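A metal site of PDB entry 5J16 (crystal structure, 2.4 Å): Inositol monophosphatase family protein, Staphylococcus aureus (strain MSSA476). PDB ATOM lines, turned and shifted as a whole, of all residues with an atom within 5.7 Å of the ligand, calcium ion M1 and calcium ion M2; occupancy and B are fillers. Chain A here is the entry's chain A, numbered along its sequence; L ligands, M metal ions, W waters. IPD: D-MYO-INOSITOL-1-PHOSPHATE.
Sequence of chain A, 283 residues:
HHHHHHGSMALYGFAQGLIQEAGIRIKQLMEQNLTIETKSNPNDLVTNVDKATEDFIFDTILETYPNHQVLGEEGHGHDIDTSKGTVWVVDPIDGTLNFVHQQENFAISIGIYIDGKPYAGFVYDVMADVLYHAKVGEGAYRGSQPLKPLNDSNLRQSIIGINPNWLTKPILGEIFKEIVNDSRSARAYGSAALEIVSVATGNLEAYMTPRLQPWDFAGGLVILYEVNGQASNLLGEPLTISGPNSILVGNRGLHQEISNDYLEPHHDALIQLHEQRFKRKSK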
ATOM      1  N   ASP A  50     -33.107  21.321   9.370  1.00  0.00           N
ATOM      2  CA  ASP A  50     -31.681  21.706   9.356  1.00  0.00           C
ATOM      3  C   ASP A  50     -31.496  23.006  10.151  1.00  0.00           C
ATOM      4  O   ASP A  50     -30.534  23.138  10.904  1.00  0.00           O
ATOM      5  CB  ASP A  50     -31.127  21.997   7.947  1.00  0.00           C
ATOM      6  CG  ASP A  50     -31.239  20.833   7.014  1.00  0.00           C
ATOM      7  OD1 ASP A  50     -30.187  20.384   6.533  1.00  0.00           O
ATOM      8  OD2 ASP A  50     -32.375  20.413   6.740  1.00  0.00           O
ATOM      9  N   GLU A  73     -23.511  25.797   7.740  1.00  0.00           N
ATOM     10  CA  GLU A  73     -24.020  25.851   6.364  1.00  0.00           C
ATOM     11  C   GLU A  73     -25.259  26.695   6.236  1.00  0.00           C
ATOM     12  O   GLU A  73     -25.316  27.586   5.387  1.00  0.00           O
ATOM     13  CB  GLU A  73     -24.176  24.456   5.730  1.00  0.00           C
ATOM     14  CG  GLU A  73     -25.546  23.779   5.673  1.00  0.00           C
ATOM     15  CD  GLU A  73     -25.730  23.063   4.356  1.00  0.00           C
ATOM     16  OE1 GLU A  73     -25.713  21.815   4.369  1.00  0.00           O
ATOM     17  OE2 GLU A  73     -25.851  23.755   3.319  1.00  0.00           O
ATOM     18  N   GLU A  74     -26.230  26.454   7.123  1.00  0.00           N
ATOM     19  CA  GLU A  74     -27.510  27.199   7.142  1.00  0.00           C
ATOM     20  C   GLU A  74     -27.364  28.598   7.784  1.00  0.00           C
ATOM     21  O   GLU A  74     -28.305  29.101   8.414  1.00  0.00           O
ATOM     22  CB  GLU A  74     -28.656  26.359   7.784  1.00  0.00           C
ATOM     23  CG  GLU A  74     -29.652  25.781   6.783  1.00  0.00           C
ATOM     24  CD  GLU A  74     -29.097  24.618   5.961  1.00  0.00           C
ATOM     25  OE1 GLU A  74     -28.534  23.678   6.550  1.00  0.00           O
ATOM     26  OE2 GLU A  74     -29.255  24.644   4.721  1.00  0.00           O
ATOM     27  N   ASP A  91     -22.203  20.979  10.158  1.00  0.00           N
ATOM     28  CA  ASP A  91     -23.222  20.621   9.202  1.00  0.00           C
ATOM     29  C   ASP A  91     -24.222  19.897  10.062  1.00  0.00           C
ATOM     30  O   ASP A  91     -23.919  18.842  10.589  1.00  0.00           O
ATOM     31  CB  ASP A  91     -22.642  19.688   8.118  1.00  0.00           C
ATOM     32  CG  ASP A  91     -23.532  19.569   6.906  1.00  0.00           C
ATOM     33  OD1 ASP A  91     -24.715  19.910   7.002  1.00  0.00           O
ATOM     34  OD2 ASP A  91     -23.016  19.079   5.861  1.00  0.00           O
ATOM     35  N   PRO A  92     -25.390  20.511  10.283  1.00  0.00           N
ATOM     36  CA  PRO A  92     -26.403  19.878  11.150  1.00  0.00           C
ATOM     37  C   PRO A  92     -27.049  18.622  10.554  1.00  0.00           C
ATOM     38  O   PRO A  92     -27.411  17.749  11.317  1.00  0.00           O
ATOM     39  CB  PRO A  92     -27.435  20.992  11.330  1.00  0.00           C
ATOM     40  CG  PRO A  92     -27.271  21.854  10.128  1.00  0.00           C
ATOM     41  CD  PRO A  92     -25.784  21.871   9.885  1.00  0.00           C
ATOM     42  N   ILE A  93     -27.236  18.544   9.236  1.00  0.00           N
ATOM     43  CA  ILE A  93     -27.662  17.296   8.565  1.00  0.00           C
ATOM     44  C   ILE A  93     -26.879  17.197   7.261  1.00  0.00           C
ATOM     45  O   ILE A  93     -27.208  17.894   6.305  1.00  0.00           O
ATOM     46  CB  ILE A  93     -29.201  17.227   8.215  1.00  0.00           C
ATOM     47  CG1 ILE A  93     -30.058  17.001   9.481  1.00  0.00           C
ATOM     48  CG2 ILE A  93     -29.507  16.071   7.260  1.00  0.00           C
ATOM     49  CD1 ILE A  93     -30.633  18.273  10.073  1.00  0.00           C
ATOM     50  N   ASP A  94     -25.840  16.353   7.256  1.00  0.00           N
ATOM     51  CA  ASP A  94     -25.144  16.008   6.048  1.00  0.00           C
ATOM     52  C   ASP A  94     -25.849  14.808   5.466  1.00  0.00           C
ATOM     53  O   ASP A  94     -25.963  13.803   6.110  1.00  0.00           O
ATOM     54  CB  ASP A  94     -23.667  15.727   6.305  1.00  0.00           C
ATOM     55  CG  ASP A  94     -22.863  15.589   4.988  1.00  0.00           C
ATOM     56  OD1 ASP A  94     -22.972  16.494   4.114  1.00  0.00           O
ATOM     57  OD2 ASP A  94     -22.171  14.563   4.810  1.00  0.00           O
ATOM     58  N   GLY A  95     -26.235  14.938   4.205  1.00  0.00           N
ATOM     59  CA  GLY A  95     -27.090  13.995   3.535  1.00  0.00           C
ATOM     60  C   GLY A  95     -28.553  14.318   3.683  1.00  0.00           C
ATOM     61  O   GLY A  95     -29.322  13.444   4.110  1.00  0.00           O
ATOM     62  N   THR A  96     -28.963  15.535   3.343  1.00  0.00           N
ATOM     63  CA  THR A  96     -30.404  15.874   3.426  1.00  0.00           C
ATOM     64  C   THR A  96     -31.289  15.108   2.441  1.00  0.00           C
ATOM     65  O   THR A  96     -32.431  14.822   2.750  1.00  0.00           O
ATOM     66  CB  THR A  96     -30.738  17.383   3.290  1.00  0.00           C
ATOM     67  OG1 THR A  96     -29.766  18.023   2.475  1.00  0.00           O
ATOM     68  CG2 THR A  96     -30.726  18.047   4.633  1.00  0.00           C
ATOM     69  N   LEU A  97     -30.768  14.783   1.264  1.00  0.00           N
ATOM     70  CA  LEU A  97     -31.523  13.956   0.320  1.00  0.00           C
ATOM     71  C   LEU A  97     -31.745  12.590   0.939  1.00  0.00           C
ATOM     72  O   LEU A  97     -32.855  12.102   0.939  1.00  0.00           O
ATOM     73  CB  LEU A  97     -30.790  13.827  -1.008  1.00  0.00           C
ATOM     74  CG  LEU A  97     -31.041  15.007  -1.909  1.00  0.00           C
ATOM     75  CD1 LEU A  97     -29.988  15.051  -3.032  1.00  0.00           C
ATOM     76  CD2 LEU A  97     -32.462  14.946  -2.488  1.00  0.00           C
ATOM     77  N   TRP A 166     -20.663  13.107 -11.177  1.00  0.00           N
ATOM     78  CA  TRP A 166     -19.376  13.688 -11.583  1.00  0.00           C
ATOM     79  C   TRP A 166     -18.876  13.168 -12.921  1.00  0.00           C
ATOM     80  O   TRP A 166     -18.113  13.855 -13.569  1.00  0.00           O
ATOM     81  CB  TRP A 166     -18.263  13.527 -10.490  1.00  0.00           C
ATOM     82  CG  TRP A 166     -18.752  13.977  -9.197  1.00  0.00           C
ATOM     83  CD1 TRP A 166     -18.741  13.274  -8.016  1.00  0.00           C
ATOM     84  CD2 TRP A 166     -19.457  15.194  -8.934  1.00  0.00           C
ATOM     85  NE1 TRP A 166     -19.350  13.998  -7.024  1.00  0.00           N
ATOM     86  CE2 TRP A 166     -19.810  15.178  -7.564  1.00  0.00           C
ATOM     87  CE3 TRP A 166     -19.785  16.306  -9.715  1.00  0.00           C
ATOM     88  CZ2 TRP A 166     -20.473  16.254  -6.940  1.00  0.00           C
ATOM     89  CZ3 TRP A 166     -20.456  17.369  -9.108  1.00  0.00           C
ATOM     90  CH2 TRP A 166     -20.784  17.338  -7.722  1.00  0.00           C
ATOM     91  N   TYR A 189     -22.806   6.856  -1.541  1.00  0.00           N
ATOM     92  CA  TYR A 189     -23.687   6.766  -0.391  1.00  0.00           C
ATOM     93  C   TYR A 189     -24.482   8.045  -0.155  1.00  0.00           C
ATOM     94  O   TYR A 189     -25.484   8.016   0.566  1.00  0.00           O
ATOM     95  CB  TYR A 189     -22.873   6.342   0.850  1.00  0.00           C
ATOM     96  CG  TYR A 189     -22.141   4.985   0.650  1.00  0.00           C
ATOM     97  CD1 TYR A 189     -22.831   3.855   0.231  1.00  0.00           C
ATOM     98  CD2 TYR A 189     -20.785   4.841   0.920  1.00  0.00           C
ATOM     99  CE1 TYR A 189     -22.199   2.631   0.071  1.00  0.00           C
ATOM    100  CE2 TYR A 189     -20.141   3.632   0.768  1.00  0.00           C
ATOM    101  CZ  TYR A 189     -20.857   2.531   0.336  1.00  0.00           C
ATOM    102  OH  TYR A 189     -20.239   1.307   0.171  1.00  0.00           O
ATOM    103  N   GLY A 190     -24.095   9.144  -0.770  1.00  0.00           N
ATOM    104  CA  GLY A 190     -24.847  10.391  -0.570  1.00  0.00           C
ATOM    105  C   GLY A 190     -24.621  11.094   0.759  1.00  0.00           C
ATOM    106  O   GLY A 190     -25.497  11.895   1.200  1.00  0.00           O
ATOM    107  N   SER A 191     -23.474  10.847   1.398  1.00  0.00           N
ATOM    108  CA  SER A 191     -23.033  11.684   2.529  1.00  0.00           C
ATOM    109  C   SER A 191     -21.537  11.832   2.504  1.00  0.00           C
ATOM    110  O   SER A 191     -20.812  10.859   2.762  1.00  0.00           O
ATOM    111  CB  SER A 191     -23.467  11.131   3.896  1.00  0.00           C
ATOM    112  OG  SER A 191     -22.786  11.778   4.977  1.00  0.00           O
ATOM    113  N   ALA A 192     -21.061  13.017   2.223  1.00  0.00           N
ATOM    114  CA  ALA A 192     -19.646  13.241   2.211  1.00  0.00           C
ATOM    115  C   ALA A 192     -19.000  12.952   3.600  1.00  0.00           C
ATOM    116  O   ALA A 192     -17.937  12.328   3.698  1.00  0.00           O
ATOM    117  CB  ALA A 192     -19.356  14.660   1.758  1.00  0.00           C
ATOM    118  N   ALA A 193     -19.650  13.403   4.665  1.00  0.00           N
ATOM    119  CA  ALA A 193     -19.107  13.172   6.000  1.00  0.00           C
ATOM    120  C   ALA A 193     -18.981  11.693   6.277  1.00  0.00           C
ATOM    121  O   ALA A 193     -17.916  11.268   6.716  1.00  0.00           O
ATOM    122  CB  ALA A 193     -19.970  13.820   7.060  1.00  0.00           C
ATOM    123  N   GLU A 195     -18.969   9.180   4.016  1.00  0.00           N
ATOM    124  CA  GLU A 195     -17.969   8.630   3.113  1.00  0.00           C
ATOM    125  C   GLU A 195     -16.517   8.871   3.464  1.00  0.00           C
ATOM    126  O   GLU A 195     -15.665   8.024   3.199  1.00  0.00           O
ATOM    127  CB  GLU A 195     -18.254   9.071   1.689  1.00  0.00           C
ATOM    128  CG  GLU A 195     -19.448   8.300   1.182  1.00  0.00           C
ATOM    129  CD  GLU A 195     -19.910   8.759  -0.125  1.00  0.00           C
ATOM    130  OE1 GLU A 195     -20.770   9.662  -0.142  1.00  0.00           O
ATOM    131  OE2 GLU A 195     -19.406   8.219  -1.110  1.00  0.00           O
ATOM    132  N   TYR A 207     -12.152   8.225  -1.593  1.00  0.00           N
ATOM    133  CA  TYR A 207     -13.379   8.954  -1.896  1.00  0.00           C
ATOM    134  C   TYR A 207     -13.009  10.253  -2.545  1.00  0.00           C
ATOM    135  O   TYR A 207     -11.975  10.822  -2.227  1.00  0.00           O
ATOM    136  CB  TYR A 207     -14.165   9.224  -0.618  1.00  0.00           C
ATOM    137  CG  TYR A 207     -15.195  10.349  -0.705  1.00  0.00           C
ATOM    138  CD1 TYR A 207     -16.320  10.254  -1.505  1.00  0.00           C
ATOM    139  CD2 TYR A 207     -15.041  11.503   0.044  1.00  0.00           C
ATOM    140  CE1 TYR A 207     -17.266  11.280  -1.565  1.00  0.00           C
ATOM    141  CE2 TYR A 207     -15.967  12.524  -0.010  1.00  0.00           C
ATOM    142  CZ  TYR A 207     -17.085  12.421  -0.810  1.00  0.00           C
ATOM    143  OH  TYR A 207     -17.993  13.468  -0.808  1.00  0.00           O
ATOM    144  N   THR A 209     -14.421  14.082  -4.821  1.00  0.00           N
ATOM    145  CA  THR A 209     -15.491  14.963  -5.262  1.00  0.00           C
ATOM    146  C   THR A 209     -14.880  16.312  -5.641  1.00  0.00           C
ATOM    147  O   THR A 209     -13.885  16.724  -5.071  1.00  0.00           O
ATOM    148  CB  THR A 209     -16.613  15.078  -4.168  1.00  0.00           C
ATOM    149  OG1 THR A 209     -17.578  16.071  -4.535  1.00  0.00           O
ATOM    150  CG2 THR A 209     -16.053  15.446  -2.847  1.00  0.00           C
ATOM    151  N   ARG A 211     -16.516  19.351  -5.418  1.00  0.00           N
ATOM    152  CA  ARG A 211     -16.963  20.432  -4.535  1.00  0.00           C
ATOM    153  C   ARG A 211     -17.487  19.946  -3.151  1.00  0.00           C
ATOM    154  O   ARG A 211     -18.525  19.298  -3.044  1.00  0.00           O
ATOM    155  CB  ARG A 211     -18.039  21.287  -5.212  1.00  0.00           C
ATOM    156  CG  ARG A 211     -18.354  22.560  -4.422  1.00  0.00           C
ATOM    157  CD  ARG A 211     -19.177  23.659  -5.138  1.00  0.00           C
ATOM    158  NE  ARG A 211     -18.911  24.968  -4.487  1.00  0.00           N
ATOM    159  CZ  ARG A 211     -18.065  25.913  -4.903  1.00  0.00           C
ATOM    160  NH1 ARG A 211     -17.399  25.798  -6.045  1.00  0.00           N
ATOM    161  NH2 ARG A 211     -17.894  27.023  -4.180  1.00  0.00           N
ATOM    162  N   LEU A 212     -16.757  20.310  -2.120  1.00  0.00           N
ATOM    163  CA  LEU A 212     -17.234  20.291  -0.760  1.00  0.00           C
ATOM    164  C   LEU A 212     -17.044  21.618  -0.022  1.00  0.00           C
ATOM    165  O   LEU A 212     -16.116  22.372  -0.315  1.00  0.00           O
ATOM    166  CB  LEU A 212     -16.478  19.193  -0.045  1.00  0.00           C
ATOM    167  CG  LEU A 212     -17.278  18.011   0.451  1.00  0.00           C
ATOM    168  CD1 LEU A 212     -18.405  17.528  -0.442  1.00  0.00           C
ATOM    169  CD2 LEU A 212     -16.326  16.874   0.844  1.00  0.00           C
ATOM    170  N   TRP A 215     -17.776  22.662   6.228  1.00  0.00           N
ATOM    171  CA  TRP A 215     -18.674  21.912   7.160  1.00  0.00           C
ATOM    172  C   TRP A 215     -18.866  20.424   6.785  1.00  0.00           C
ATOM    173  O   TRP A 215     -19.176  19.594   7.652  1.00  0.00           O
ATOM    174  CB  TRP A 215     -20.025  22.620   7.362  1.00  0.00           C
ATOM    175  CG  TRP A 215     -20.678  23.176   6.121  1.00  0.00           C
ATOM    176  CD1 TRP A 215     -21.457  22.494   5.236  1.00  0.00           C
ATOM    177  CD2 TRP A 215     -20.577  24.513   5.617  1.00  0.00           C
ATOM    178  NE1 TRP A 215     -21.839  23.317   4.205  1.00  0.00           N
ATOM    179  CE2 TRP A 215     -21.327  24.565   4.417  1.00  0.00           C
ATOM    180  CE3 TRP A 215     -19.901  25.675   6.049  1.00  0.00           C
ATOM    181  CZ2 TRP A 215     -21.448  25.755   3.639  1.00  0.00           C
ATOM    182  CZ3 TRP A 215     -19.997  26.850   5.287  1.00  0.00           C
ATOM    183  CH2 TRP A 215     -20.771  26.876   4.095  1.00  0.00           C
ATOM    184  N   ASP A 216     -18.673  20.085   5.514  1.00  0.00           N
ATOM    185  CA  ASP A 216     -18.800  18.687   5.051  1.00  0.00           C
ATOM    186  C   ASP A 216     -17.584  17.825   5.439  1.00  0.00           C
ATOM    187  O   ASP A 216     -17.719  16.613   5.625  1.00  0.00           O
ATOM    188  CB  ASP A 216     -18.998  18.596   3.509  1.00  0.00           C
ATOM    189  CG  ASP A 216     -20.319  19.239   3.012  1.00  0.00           C
ATOM    190  OD1 ASP A 216     -20.273  19.942   1.927  1.00  0.00           O
ATOM    191  OD2 ASP A 216     -21.384  19.041   3.672  1.00  0.00           O
HETATM  192  C1  IPD L   1     -24.222  17.201   0.546  1.00  0.00           C
HETATM  193  C2  IPD L   1     -23.817  15.769   0.877  1.00  0.00           C
HETATM  194  C3  IPD L   1     -23.716  15.017  -0.481  1.00  0.00           C
HETATM  195  C4  IPD L   1     -22.624  15.598  -1.376  1.00  0.00           C
HETATM  196  C5  IPD L   1     -22.858  17.094  -1.644  1.00  0.00           C
HETATM  197  C6  IPD L   1     -23.100  17.883  -0.293  1.00  0.00           C
HETATM  198  P1  IPD L   1     -26.041  18.265   2.265  1.00  0.00           P
HETATM  199  O1  IPD L   1     -24.501  17.968   1.705  1.00  0.00           O
HETATM  200  O2  IPD L   1     -22.545  15.744   1.590  1.00  0.00           O
HETATM  201  O3  IPD L   1     -23.488  13.632  -0.330  1.00  0.00           O
HETATM  202  O4  IPD L   1     -22.684  14.983  -2.627  1.00  0.00           O
HETATM  203  O5  IPD L   1     -21.685  17.554  -2.334  1.00  0.00           O
HETATM  204  O6  IPD L   1     -23.514  19.192  -0.591  1.00  0.00           O
HETATM  205  O7  IPD L   1     -26.853  19.228   1.444  1.00  0.00           O
HETATM  206  O8  IPD L   1     -26.778  16.811   2.349  1.00  0.00           O
HETATM  207  O9  IPD L   1     -25.772  18.762   3.808  1.00  0.00           O
HETATM  208 CA    CA M   1     -26.630  20.197   5.534  1.00  0.00          CA
HETATM  209 CA    CA M   2     -23.455  18.773   3.719  1.00  0.00          CA
HETATM  210  O   HOH W   1     -24.250  12.860  -2.943  1.00  0.00           O
HETATM  211  O   HOH W   2     -27.643  15.240   0.053  1.00  0.00           O
HETATM  212  O   HOH W   3     -23.359  21.022   2.833  1.00  0.00           O
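The backbone NH (N) of Ser 191 sits at hydrogen-bond distance from an oxygen (O3) of the ligand, 3.3 Å away.
N of Thr 96 sits at hydrogen-bond distance from O8 of the ligand (2.7 Å).
An oxygen (O8) of the ligand is in hydrogen-bond range of the side-chain hydroxyl (OG1) of Thr 96 (3.2 Å).
An oxygen (O2) of the ligand is in hydrogen-bond range of the backbone NH (N) of Ala 192, at 3.2 Å.
O8 of the ligand lies within hydrogen-bond range of N of Gly 95.
O of Gly 190 lies close to O3 of the ligand (3.1 Å).
The side-chain carboxylate (OD2) of Asp 94 lies within hydrogen-bond range of the side-chain hydroxyl (OG) of Ser 191 (2.9 Å).
N of Ser 191 lies within hydrogen-bond range of OE1 of Glu 195.
OD2 of Asp 94 lies within hydrogen-bond range of N of Ala 193 (2.8 Å).
The backbone NH (N) of Ala 192 lies within hydrogen-bond range of the side-chain carboxylate (OD2) of Asp 94 (3.2 Å).
The side-chain carboxylate of Glu 195 sits at hydrogen-bond distance from the backbone NH of Gly 190, 3.4 Å away.
Merely in contact with the ligand: Arg 211 and Leu 212.
Hydrophobic or aromatic side chains within 4 Å of the ligand: Ala 192 and Leu 212.
Merely in contact with calcium ion M1: Asp 50 (3.7 Å).
Four residues have an atom within 4 Å of calcium ion M1: Asp 50, Glu 73, Asp 91 and Ile 93.
The nearest printed residue that does not touch calcium ion M1 is Glu 74 (4.1 Å).
Four residues have an atom within 4 Å of calcium ion M2: Glu 73, Asp 91, Asp 94 and Asp 216.
Along chain A the residues within 4 Å of calcium ion M2 span positions 73 to 216.
The nearest printed residue that does not touch calcium ion M2 is Trp 215 (4.5 Å).
Calcium ion M1 is bound by the side-chain carboxylate (OE1) of Glu 73, an oxygen (O9) of the ligand, the side-chain carboxylate (OD1) of Asp 91 and the backbone carbonyl oxygen (O) of Ile 93.
Calcium ion M2 is bound by the side-chain carboxylate (OD2) of Asp 216 (2.1 Å).
Calcium ion M2 is bound by OD2 of Asp 91 (2.2 Å).
An oxygen (O9) of the ligand binds calcium ion M2.
Calcium ion M2 is bound by OD1 of Asp 94 (2.4 Å).
O1 of the ligand is bound to calcium ion M2, 2.4 Å away.
Calcium ion M2 is bound by water W3 (2.4 Å).
Calcium ion M2 has six donor atoms within binding distance.
Water W3 bridges NE1 of Trp 215 (3.1 Å) and OD1 of Asp 216 (3.4 Å).
Water W2 bridges an oxygen (O8) of the ligand (2.9 Å) and the backbone NH of Leu 97 (3.4 Å).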
